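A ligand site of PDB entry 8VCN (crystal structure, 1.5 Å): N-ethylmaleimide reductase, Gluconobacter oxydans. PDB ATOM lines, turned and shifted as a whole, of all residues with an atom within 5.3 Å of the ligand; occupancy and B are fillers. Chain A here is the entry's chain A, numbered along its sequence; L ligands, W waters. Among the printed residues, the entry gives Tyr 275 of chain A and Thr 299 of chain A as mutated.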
ATOM      1  N   SER A  28     -24.228   4.979 -26.747  1.00  0.00           N
ATOM      2  CA  SER A  28     -24.534   3.919 -25.807  1.00  0.00           C
ATOM      3  C   SER A  28     -24.700   2.586 -26.542  1.00  0.00           C
ATOM      4  O   SER A  28     -24.917   2.551 -27.743  1.00  0.00           O
ATOM      5  CB  SER A  28     -25.782   4.275 -24.996  1.00  0.00           C
ATOM      6  OG  SER A  28     -26.973   3.798 -25.605  1.00  0.00           O
ATOM      7  N   PRO A  29     -24.577   1.459 -25.819  1.00  0.00           N
ATOM      8  CA  PRO A  29     -24.677   0.146 -26.466  1.00  0.00           C
ATOM      9  C   PRO A  29     -26.101  -0.124 -26.947  1.00  0.00           C
ATOM     10  O   PRO A  29     -27.065   0.029 -26.193  1.00  0.00           O
ATOM     11  CB  PRO A  29     -24.299  -0.813 -25.339  1.00  0.00           C
ATOM     12  CG  PRO A  29     -24.637  -0.070 -24.071  1.00  0.00           C
ATOM     13  CD  PRO A  29     -24.238   1.349 -24.384  1.00  0.00           C
ATOM     14  N   LEU A  30     -26.229  -0.563 -28.200  1.00  0.00           N
ATOM     15  CA  LEU A  30     -27.539  -0.778 -28.823  1.00  0.00           C
ATOM     16  C   LEU A  30     -27.551  -2.069 -29.616  1.00  0.00           C
ATOM     17  O   LEU A  30     -26.961  -2.153 -30.689  1.00  0.00           O
ATOM     18  CB  LEU A  30     -27.911   0.398 -29.718  1.00  0.00           C
ATOM     19  CG  LEU A  30     -28.016   1.767 -29.057  1.00  0.00           C
ATOM     20  CD1 LEU A  30     -27.808   2.837 -30.112  1.00  0.00           C
ATOM     21  CD2 LEU A  30     -29.374   1.909 -28.394  1.00  0.00           C
ATOM     22  N   THR A  31     -28.254  -3.082 -29.097  1.00  0.00           N
ATOM     23  CA  THR A  31     -28.498  -4.305 -29.838  1.00  0.00           C
ATOM     24  C   THR A  31     -29.344  -3.997 -31.069  1.00  0.00           C
ATOM     25  O   THR A  31     -30.395  -3.353 -30.964  1.00  0.00           O
ATOM     26  CB  THR A  31     -29.257  -5.260 -28.906  1.00  0.00           C
ATOM     27  OG1 THR A  31     -28.354  -5.732 -27.899  1.00  0.00           O
ATOM     28  CG2 THR A  31     -29.808  -6.457 -29.662  1.00  0.00           C
ATOM     29  N   ARG A  32     -28.890  -4.448 -32.240  1.00  0.00           N
ATOM     30  CA  ARG A  32     -29.607  -4.172 -33.488  1.00  0.00           C
ATOM     31  C   ARG A  32     -29.918  -5.407 -34.310  1.00  0.00           C
ATOM     32  O   ARG A  32     -30.754  -5.329 -35.222  1.00  0.00           O
ATOM     33  CB  ARG A  32     -28.830  -3.176 -34.368  1.00  0.00           C
ATOM     34  CG  ARG A  32     -28.401  -1.884 -33.645  1.00  0.00           C
ATOM     35  CD  ARG A  32     -29.614  -1.118 -33.094  1.00  0.00           C
ATOM     36  NE  ARG A  32     -30.616  -0.847 -34.125  1.00  0.00           N
ATOM     37  CZ  ARG A  32     -30.513   0.113 -35.035  1.00  0.00           C
ATOM     38  NH1 ARG A  32     -31.477   0.281 -35.931  1.00  0.00           N
ATOM     39  NH2 ARG A  32     -29.438   0.913 -35.055  1.00  0.00           N
ATOM     40  N   THR A  60     -20.187  -0.791 -28.311  1.00  0.00           N
ATOM     41  CA  THR A  60     -20.933  -1.608 -29.258  1.00  0.00           C
ATOM     42  C   THR A  60     -22.226  -2.131 -28.630  1.00  0.00           C
ATOM     43  O   THR A  60     -22.395  -2.195 -27.410  1.00  0.00           O
ATOM     44  CB  THR A  60     -20.169  -2.866 -29.706  1.00  0.00           C
ATOM     45  OG1 THR A  60     -19.992  -3.769 -28.594  1.00  0.00           O
ATOM     46  CG2 THR A  60     -18.840  -2.503 -30.347  1.00  0.00           C
ATOM     47  N   GLU A  61     -23.121  -2.554 -29.520  1.00  0.00           N
ATOM     48  CA  GLU A  61     -24.147  -3.520 -29.161  1.00  0.00           C
ATOM     49  C   GLU A  61     -23.599  -4.599 -28.244  1.00  0.00           C
ATOM     50  O   GLU A  61     -22.440  -5.019 -28.344  1.00  0.00           O
ATOM     51  CB  GLU A  61     -24.689  -4.177 -30.426  1.00  0.00           C
ATOM     52  CG  GLU A  61     -23.699  -5.055 -31.163  1.00  0.00           C
ATOM     53  CD  GLU A  61     -23.988  -5.097 -32.646  1.00  0.00           C
ATOM     54  OE1 GLU A  61     -23.480  -4.221 -33.376  1.00  0.00           O
ATOM     55  OE2 GLU A  61     -24.742  -6.003 -33.071  1.00  0.00           O
ATOM     56  N   ALA A  62     -24.462  -5.099 -27.363  1.00  0.00           N
ATOM     57  CA  ALA A  62     -24.069  -6.188 -26.496  1.00  0.00           C
ATOM     58  C   ALA A  62     -23.618  -7.385 -27.339  1.00  0.00           C
ATOM     59  O   ALA A  62     -24.245  -7.722 -28.343  1.00  0.00           O
ATOM     60  CB  ALA A  62     -25.273  -6.560 -25.644  1.00  0.00           C
ATOM     61  N   GLN A 104     -18.992  -4.258 -25.759  1.00  0.00           N
ATOM     62  CA  GLN A 104     -19.779  -4.585 -24.579  1.00  0.00           C
ATOM     63  C   GLN A 104     -19.938  -6.100 -24.495  1.00  0.00           C
ATOM     64  O   GLN A 104     -20.552  -6.709 -25.370  1.00  0.00           O
ATOM     65  CB  GLN A 104     -21.167  -3.939 -24.621  1.00  0.00           C
ATOM     66  CG  GLN A 104     -21.880  -4.149 -23.289  1.00  0.00           C
ATOM     67  CD  GLN A 104     -23.325  -3.666 -23.265  1.00  0.00           C
ATOM     68  OE1 GLN A 104     -24.152  -4.083 -24.067  1.00  0.00           O
ATOM     69  NE2 GLN A 104     -23.629  -2.801 -22.309  1.00  0.00           N
ATOM     70  N   HIS A 178     -21.105  -5.819 -19.451  1.00  0.00           N
ATOM     71  CA  HIS A 178     -22.548  -5.575 -19.323  1.00  0.00           C
ATOM     72  C   HIS A 178     -22.974  -6.187 -18.000  1.00  0.00           C
ATOM     73  O   HIS A 178     -23.175  -7.392 -17.885  1.00  0.00           O
ATOM     74  CB  HIS A 178     -23.303  -6.202 -20.489  1.00  0.00           C
ATOM     75  CG  HIS A 178     -24.706  -5.712 -20.623  1.00  0.00           C
ATOM     76  ND1 HIS A 178     -25.391  -5.079 -19.610  1.00  0.00           N
ATOM     77  CD2 HIS A 178     -25.564  -5.757 -21.679  1.00  0.00           C
ATOM     78  CE1 HIS A 178     -26.597  -4.757 -20.028  1.00  0.00           C
ATOM     79  NE2 HIS A 178     -26.739  -5.176 -21.276  1.00  0.00           N
ATOM     80  N   ASN A 181     -29.309  -4.385 -16.759  1.00  0.00           N
ATOM     81  CA  ASN A 181     -30.505  -4.662 -17.551  1.00  0.00           C
ATOM     82  C   ASN A 181     -31.067  -6.066 -17.334  1.00  0.00           C
ATOM     83  O   ASN A 181     -31.707  -6.630 -18.220  1.00  0.00           O
ATOM     84  CB  ASN A 181     -30.332  -4.322 -19.033  1.00  0.00           C
ATOM     85  CG  ASN A 181     -29.953  -2.879 -19.227  1.00  0.00           C
ATOM     86  OD1 ASN A 181     -30.099  -2.065 -18.319  1.00  0.00           O
ATOM     87  ND2 ASN A 181     -29.452  -2.544 -20.412  1.00  0.00           N
ATOM     88  N   ARG A 230     -21.046  -1.261 -17.196  1.00  0.00           N
ATOM     89  CA  ARG A 230     -22.362  -0.629 -17.157  1.00  0.00           C
ATOM     90  C   ARG A 230     -23.178  -1.249 -16.032  1.00  0.00           C
ATOM     91  O   ARG A 230     -23.269  -2.482 -15.944  1.00  0.00           O
ATOM     92  CB  ARG A 230     -23.143  -0.823 -18.463  1.00  0.00           C
ATOM     93  CG  ARG A 230     -24.584  -0.293 -18.368  1.00  0.00           C
ATOM     94  CD  ARG A 230     -25.341  -0.406 -19.708  1.00  0.00           C
ATOM     95  NE  ARG A 230     -25.372   0.863 -20.435  1.00  0.00           N
ATOM     96  CZ  ARG A 230     -26.412   1.255 -21.174  1.00  0.00           C
ATOM     97  NH1 ARG A 230     -27.472   0.459 -21.273  1.00  0.00           N
ATOM     98  NH2 ARG A 230     -26.403   2.434 -21.794  1.00  0.00           N
ATOM     99  N   ARG A 267     -27.122   3.424 -16.563  1.00  0.00           N
ATOM    100  CA  ARG A 267     -28.429   3.581 -17.178  1.00  0.00           C
ATOM    101  C   ARG A 267     -29.415   3.873 -16.044  1.00  0.00           C
ATOM    102  O   ARG A 267     -29.636   3.008 -15.195  1.00  0.00           O
ATOM    103  CB  ARG A 267     -28.826   2.306 -17.926  1.00  0.00           C
ATOM    104  CG  ARG A 267     -30.305   2.267 -18.340  1.00  0.00           C
ATOM    105  CD  ARG A 267     -30.619   1.173 -19.372  1.00  0.00           C
ATOM    106  NE  ARG A 267     -32.050   1.160 -19.637  1.00  0.00           N
ATOM    107  CZ  ARG A 267     -32.924   0.370 -19.017  1.00  0.00           C
ATOM    108  NH1 ARG A 267     -34.221   0.484 -19.287  1.00  0.00           N
ATOM    109  NH2 ARG A 267     -32.507  -0.544 -18.149  1.00  0.00           N
ATOM    110  N   TYR A 275     -37.953   4.691 -21.951  1.00  0.00           N
ATOM    111  CA  TYR A 275     -37.515   3.329 -22.222  1.00  0.00           C
ATOM    112  C   TYR A 275     -37.305   2.661 -20.860  1.00  0.00           C
ATOM    113  O   TYR A 275     -36.184   2.362 -20.447  1.00  0.00           O
ATOM    114  CB  TYR A 275     -36.255   3.293 -23.102  1.00  0.00           C
ATOM    115  CG  TYR A 275     -35.872   1.889 -23.522  1.00  0.00           C
ATOM    116  CD1 TYR A 275     -36.685   1.158 -24.374  1.00  0.00           C
ATOM    117  CD2 TYR A 275     -34.715   1.290 -23.035  1.00  0.00           C
ATOM    118  CE1 TYR A 275     -36.365  -0.140 -24.748  1.00  0.00           C
ATOM    119  CE2 TYR A 275     -34.375  -0.012 -23.399  1.00  0.00           C
ATOM    120  CZ  TYR A 275     -35.202  -0.716 -24.253  1.00  0.00           C
ATOM    121  OH  TYR A 275     -34.884  -2.000 -24.628  1.00  0.00           O
ATOM    122  N   ASN A 298     -26.700   7.937 -18.520  1.00  0.00           N
ATOM    123  CA  ASN A 298     -27.491   7.561 -19.696  1.00  0.00           C
ATOM    124  C   ASN A 298     -28.954   7.434 -19.314  1.00  0.00           C
ATOM    125  O   ASN A 298     -29.279   7.021 -18.202  1.00  0.00           O
ATOM    126  CB  ASN A 298     -27.035   6.205 -20.250  1.00  0.00           C
ATOM    127  CG  ASN A 298     -28.071   5.589 -21.171  1.00  0.00           C
ATOM    128  OD1 ASN A 298     -28.883   4.764 -20.734  1.00  0.00           O
ATOM    129  ND2 ASN A 298     -28.059   5.992 -22.440  1.00  0.00           N
ATOM    130  N   THR A 299     -29.816   7.813 -20.285  1.00  0.00           N
ATOM    131  CA  THR A 299     -31.263   7.612 -20.384  1.00  0.00           C
ATOM    132  C   THR A 299     -32.018   8.933 -20.357  1.00  0.00           C
ATOM    133  O   THR A 299     -31.931   9.677 -19.366  1.00  0.00           O
ATOM    134  CB  THR A 299     -31.867   6.633 -19.366  1.00  0.00           C
ATOM    135  OG1 THR A 299     -31.431   5.285 -19.638  1.00  0.00           O
ATOM    136  CG2 THR A 299     -33.379   6.658 -19.458  1.00  0.00           C
ATOM    137  N   ASP A 300     -32.753   9.227 -21.423  1.00  0.00           N
ATOM    138  CA  ASP A 300     -33.695  10.347 -21.447  1.00  0.00           C
ATOM    139  C   ASP A 300     -33.013  11.693 -21.211  1.00  0.00           C
ATOM    140  O   ASP A 300     -33.556  12.563 -20.524  1.00  0.00           O
ATOM    141  CB  ASP A 300     -34.844  10.146 -20.448  1.00  0.00           C
ATOM    142  CG  ASP A 300     -35.879   9.139 -20.940  1.00  0.00           C
ATOM    143  OD1 ASP A 300     -36.056   8.994 -22.162  1.00  0.00           O
ATOM    144  OD2 ASP A 300     -36.544   8.509 -20.086  1.00  0.00           O
ATOM    145  N   TYR A 301     -31.822  11.868 -21.753  1.00  0.00           N
ATOM    146  CA  TYR A 301     -31.145  13.156 -21.710  1.00  0.00           C
ATOM    147  C   TYR A 301     -31.442  13.959 -22.959  1.00  0.00           C
ATOM    148  O   TYR A 301     -31.082  13.540 -24.072  1.00  0.00           O
ATOM    149  CB  TYR A 301     -29.634  12.975 -21.587  1.00  0.00           C
ATOM    150  CG  TYR A 301     -29.174  12.761 -20.169  1.00  0.00           C
ATOM    151  CD1 TYR A 301     -28.913  13.846 -19.337  1.00  0.00           C
ATOM    152  CD2 TYR A 301     -29.031  11.479 -19.647  1.00  0.00           C
ATOM    153  CE1 TYR A 301     -28.512  13.655 -18.035  1.00  0.00           C
ATOM    154  CE2 TYR A 301     -28.631  11.287 -18.345  1.00  0.00           C
ATOM    155  CZ  TYR A 301     -28.365  12.379 -17.549  1.00  0.00           C
ATOM    156  OH  TYR A 301     -27.974  12.193 -16.255  1.00  0.00           O
ATOM    157  N   ALA A 319     -23.959   9.269 -22.394  1.00  0.00           N
ATOM    158  CA  ALA A 319     -24.135   8.329 -23.487  1.00  0.00           C
ATOM    159  C   ALA A 319     -25.565   8.400 -24.004  1.00  0.00           C
ATOM    160  O   ALA A 319     -26.518   8.397 -23.231  1.00  0.00           O
ATOM    161  CB  ALA A 319     -23.828   6.897 -23.026  1.00  0.00           C
ATOM    162  N   PHE A 320     -25.700   8.472 -25.324  1.00  0.00           N
ATOM    163  CA  PHE A 320     -26.992   8.566 -25.972  1.00  0.00           C
ATOM    164  C   PHE A 320     -27.208   7.301 -26.793  1.00  0.00           C
ATOM    165  O   PHE A 320     -26.316   6.881 -27.539  1.00  0.00           O
ATOM    166  CB  PHE A 320     -27.039   9.775 -26.892  1.00  0.00           C
ATOM    167  CG  PHE A 320     -26.816  11.087 -26.178  1.00  0.00           C
ATOM    168  CD1 PHE A 320     -25.538  11.595 -26.007  1.00  0.00           C
ATOM    169  CD2 PHE A 320     -27.891  11.820 -25.699  1.00  0.00           C
ATOM    170  CE1 PHE A 320     -25.321  12.803 -25.362  1.00  0.00           C
ATOM    171  CE2 PHE A 320     -27.685  13.034 -25.049  1.00  0.00           C
ATOM    172  CZ  PHE A 320     -26.394  13.529 -24.891  1.00  0.00           C
ATOM    173  N   GLY A 321     -28.385   6.719 -26.648  1.00  0.00           N
ATOM    174  CA  GLY A 321     -28.775   5.553 -27.418  1.00  0.00           C
ATOM    175  C   GLY A 321     -29.640   5.874 -28.610  1.00  0.00           C
ATOM    176  O   GLY A 321     -29.148   5.945 -29.741  1.00  0.00           O
ATOM    177  N   ARG A 322     -30.932   6.108 -28.381  1.00  0.00           N
ATOM    178  CA  ARG A 322     -31.860   6.294 -29.479  1.00  0.00           C
ATOM    179  C   ARG A 322     -31.475   7.468 -30.382  1.00  0.00           C
ATOM    180  O   ARG A 322     -31.654   7.402 -31.598  1.00  0.00           O
ATOM    181  CB  ARG A 322     -33.304   6.396 -28.963  1.00  0.00           C
ATOM    182  CG  ARG A 322     -33.834   5.044 -28.449  1.00  0.00           C
ATOM    183  CD  ARG A 322     -35.055   5.221 -27.560  1.00  0.00           C
ATOM    184  NE  ARG A 322     -34.671   5.841 -26.288  1.00  0.00           N
ATOM    185  CZ  ARG A 322     -35.531   6.216 -25.352  1.00  0.00           C
ATOM    186  NH1 ARG A 322     -36.836   6.053 -25.554  1.00  0.00           N
ATOM    187  NH2 ARG A 322     -35.095   6.753 -24.215  1.00  0.00           N
ATOM    188  N   LYS A 323     -30.931   8.549 -29.817  1.00  0.00           N
ATOM    189  CA  LYS A 323     -30.490   9.646 -30.668  1.00  0.00           C
ATOM    190  C   LYS A 323     -29.410   9.215 -31.658  1.00  0.00           C
ATOM    191  O   LYS A 323     -29.391   9.711 -32.786  1.00  0.00           O
ATOM    192  CB  LYS A 323     -30.031  10.854 -29.846  1.00  0.00           C
ATOM    193  CG  LYS A 323     -31.176  11.640 -29.222  1.00  0.00           C
ATOM    194  CD  LYS A 323     -30.689  12.728 -28.251  1.00  0.00           C
ATOM    195  CE  LYS A 323     -31.850  13.394 -27.520  1.00  0.00           C
ATOM    196  NZ  LYS A 323     -32.465  12.485 -26.504  1.00  0.00           N
ATOM    197  N   ILE A 325     -29.155   6.163 -32.960  1.00  0.00           N
ATOM    198  CA  ILE A 325     -29.775   5.325 -33.982  1.00  0.00           C
ATOM    199  C   ILE A 325     -30.078   6.156 -35.218  1.00  0.00           C
ATOM    200  O   ILE A 325     -29.734   5.784 -36.341  1.00  0.00           O
ATOM    201  CB  ILE A 325     -31.048   4.660 -33.421  1.00  0.00           C
ATOM    202  CG1 ILE A 325     -30.693   3.637 -32.353  1.00  0.00           C
ATOM    203  CG2 ILE A 325     -31.857   4.012 -34.537  1.00  0.00           C
ATOM    204  CD1 ILE A 325     -31.919   3.016 -31.736  1.00  0.00           C
ATOM    205  N   TRP A 348     -35.621  -1.021 -35.019  1.00  0.00           N
ATOM    206  CA  TRP A 348     -34.575  -1.215 -34.026  1.00  0.00           C
ATOM    207  C   TRP A 348     -33.907  -2.582 -34.179  1.00  0.00           C
ATOM    208  O   TRP A 348     -32.681  -2.708 -34.125  1.00  0.00           O
ATOM    209  CB  TRP A 348     -35.163  -1.111 -32.618  1.00  0.00           C
ATOM    210  CG  TRP A 348     -35.444   0.283 -32.111  1.00  0.00           C
ATOM    211  CD1 TRP A 348     -35.202   1.468 -32.727  1.00  0.00           C
ATOM    212  CD2 TRP A 348     -36.035   0.596 -30.835  1.00  0.00           C
ATOM    213  NE1 TRP A 348     -35.605   2.519 -31.924  1.00  0.00           N
ATOM    214  CE2 TRP A 348     -36.128   2.009 -30.752  1.00  0.00           C
ATOM    215  CE3 TRP A 348     -36.495  -0.174 -29.758  1.00  0.00           C
ATOM    216  CZ2 TRP A 348     -36.658   2.668 -29.632  1.00  0.00           C
ATOM    217  CZ3 TRP A 348     -37.002   0.468 -28.641  1.00  0.00           C
ATOM    218  CH2 TRP A 348     -37.089   1.873 -28.593  1.00  0.00           C
ATOM    219  N   TYR A 349     -34.717  -3.623 -34.345  1.00  0.00           N
ATOM    220  CA  TYR A 349     -34.245  -4.995 -34.254  1.00  0.00           C
ATOM    221  C   TYR A 349     -34.542  -5.809 -35.503  1.00  0.00           C
ATOM    222  O   TYR A 349     -34.432  -7.036 -35.465  1.00  0.00           O
ATOM    223  CB  TYR A 349     -34.914  -5.698 -33.072  1.00  0.00           C
ATOM    224  CG  TYR A 349     -34.731  -5.047 -31.715  1.00  0.00           C
ATOM    225  CD1 TYR A 349     -33.480  -4.934 -31.134  1.00  0.00           C
ATOM    226  CD2 TYR A 349     -35.826  -4.607 -30.991  1.00  0.00           C
ATOM    227  CE1 TYR A 349     -33.320  -4.369 -29.886  1.00  0.00           C
ATOM    228  CE2 TYR A 349     -35.679  -4.029 -29.731  1.00  0.00           C
ATOM    229  CZ  TYR A 349     -34.421  -3.938 -29.185  1.00  0.00           C
ATOM    230  OH  TYR A 349     -34.260  -3.373 -27.937  1.00  0.00           O
HETATM  231  N1  LIG L   1     -28.301  -1.395 -23.363  1.00  0.00           N
HETATM  232  C1  LIG L   1     -27.225  -2.233 -23.211  1.00  0.00           C
HETATM  233  O1  LIG L   1     -26.578  -2.191 -22.171  1.00  0.00           O
HETATM  234  N2  LIG L   1     -26.852  -3.110 -24.207  1.00  0.00           N
HETATM  235  C2  LIG L   1     -27.547  -3.186 -25.375  1.00  0.00           C
HETATM  236  O2  LIG L   1     -27.181  -3.989 -26.259  1.00  0.00           O
HETATM  237  C3  LIG L   1     -28.651  -2.353 -25.545  1.00  0.00           C
HETATM  238  N3  LIG L   1     -29.380  -2.411 -26.710  1.00  0.00           N
HETATM  239  C4  LIG L   1     -30.434  -1.557 -26.888  1.00  0.00           C
HETATM  240  C5  LIG L   1     -31.131  -1.591 -28.086  1.00  0.00           C
HETATM  241  C6  LIG L   1     -32.203  -0.740 -28.280  1.00  0.00           C
HETATM  242  C7  LIG L   1     -32.940  -0.826 -29.582  1.00  0.00           C
HETATM  243  C8  LIG L   1     -32.549   0.170 -27.295  1.00  0.00           C
HETATM  244  C9  LIG L   1     -33.714   1.107 -27.504  1.00  0.00           C
HETATM  245  C10 LIG L   1     -31.853   0.218 -26.098  1.00  0.00           C
HETATM  246  C11 LIG L   1     -30.781  -0.633 -25.904  1.00  0.00           C
HETATM  247  N4  LIG L   1     -30.082  -0.613 -24.706  1.00  0.00           N
HETATM  248  C12 LIG L   1     -29.008  -1.451 -24.540  1.00  0.00           C
HETATM  249  C13 LIG L   1     -30.342   0.419 -23.661  1.00  0.00           C
HETATM  250  C14 LIG L   1     -29.604   1.663 -24.237  1.00  0.00           C
HETATM  251  O3  LIG L   1     -28.170   1.566 -24.240  1.00  0.00           O
HETATM  252  C15 LIG L   1     -29.963   2.955 -23.496  1.00  0.00           C
HETATM  253  O4  LIG L   1     -29.782   2.720 -22.110  1.00  0.00           O
HETATM  254  C16 LIG L   1     -31.404   3.399 -23.757  1.00  0.00           C
HETATM  255  O5  LIG L   1     -31.594   3.503 -25.157  1.00  0.00           O
HETATM  256  C17 LIG L   1     -31.763   4.739 -23.067  1.00  0.00           C
HETATM  257  O6  LIG L   1     -30.863   5.764 -23.466  1.00  0.00           O
HETATM  258  P1  LIG L   1     -31.386   6.893 -24.474  1.00  0.00           P
HETATM  259  O7  LIG L   1     -30.181   7.766 -24.770  1.00  0.00           O
HETATM  260  O8  LIG L   1     -32.528   7.658 -23.841  1.00  0.00           O
HETATM  261  O9  LIG L   1     -31.891   6.170 -25.718  1.00  0.00           O
HETATM  262  O   HOH W   1     -29.181   9.265 -22.714  1.00  0.00           O
HETATM  263  O   HOH W   2     -33.476   3.476 -20.579  1.00  0.00           O
HETATM  264  O   HOH W   3     -30.736   9.242 -27.031  1.00  0.00           O
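Water W1 lies within hydrogen-bond range of O7 of the ligand (2.7 Å), O of Ala 319 (2.8 Å), N of Thr 299 (2.9 Å) and ND2 of Asn 298 (3.5 Å). Water W2 lies within hydrogen-bond range of the guanidinium group of Arg 267 (2.9 Å), the side-chain hydroxyl of Thr 299 (2.9 Å) and the backbone carbonyl oxygen of Tyr 275 (2.9 Å).
Residues that only touch the ligand: Leu 30, Arg 267, Tyr 275, Thr 299, Phe 320, Trp 348 and Tyr 349. Hydrophobic or aromatic side chains that line the ligand: Pro 29, Leu 30, Ala 62, His 178, Tyr 275, Trp 348 and Tyr 349. Within 4 Å of the ligand: Ser 28, Pro 29, Leu 30, Thr 31, Ala 62, Gln 104, His 178, Asn 181, Arg 230, Arg 267, Tyr 275, Asn 298, Thr 299, Asp 300, Phe 320, Gly 321, Arg 322, Trp 348 and Tyr 349. The nearest printed residue that does not touch the ligand is Ala 319 (4.02 Å).
The side-chain amide oxygen (OD1) of Asn 298 is in hydrogen-bond range of an oxygen (O4) of the ligand. The backbone NH (N) of Thr 31 is in hydrogen-bond range of a nitrogen (N3) of the ligand (2.7 Å). An oxygen (O2) of the ligand sits at hydrogen-bond distance from the side-chain hydroxyl (OG1) of Thr 31 (2.7 Å). The backbone carbonyl oxygen (O) of Pro 29 is in hydrogen-bond range of an oxygen (O3) of the ligand. An oxygen (O9) of the ligand lies within hydrogen-bond range of the backbone NH (N) of Arg 322, 2.8 Å away. NH2 of Arg 322 lies within salt-bridge range of O8 of the ligand (2.7 Å). An oxygen (O7) of the ligand is in hydrogen-bond range of the backbone NH of Gly 321 (2.8 Å). The side-chain amide oxygen of Gln 104 is in hydrogen-bond range of a nitrogen (N2) of the ligand, at 2.9 Å. O3 of the ligand lies within hydrogen-bond range of OG of Ser 28, at 2.9 Å. N of Asp 300 is in hydrogen-bond range of O8 of the ligand. NH1 of Arg 230 is in hydrogen-bond range of N1 of the ligand (2.9 Å). O1 of the ligand is in hydrogen-bond range of NE2 of His 178 (3.1 Å). An oxygen (O2) of the ligand is in hydrogen-bond range of the backbone NH (N) of Ala 62 (3.1 Å). N1 of the ligand is in hydrogen-bond range of ND2 of Asn 181, 3.4 Å away.
The side-chain amide oxygen (OD1) of Asn 298 sits at hydrogen-bond distance from the side-chain hydroxyl (OG1) of Thr 299 (2.8 Å). The guanidinium group (NH2) of Arg 322 lies within salt-bridge range of the side-chain carboxylate (OD1) of Asp 300, at 3.2 Å. N of Gly 321 sits close to OG of Ser 28. OG1 of Thr 60 lies within hydrogen-bond range of N of Gln 104, 3.0 Å away. N of Ser 28 sits at hydrogen-bond distance from O of Phe 320 (2.9 Å). The guanidinium group (NH2) of Arg 267 lies within hydrogen-bond range of the side-chain amide oxygen (OD1) of Asn 181 (2.9 Å). NH1 of Arg 267 sits at hydrogen-bond distance from O of Tyr 275 (3.0 Å). The backbone carbonyl oxygen (O) of Trp 348 lies within hydrogen-bond range of the guanidinium group (NE) of Arg 32, at 2.8 Å.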
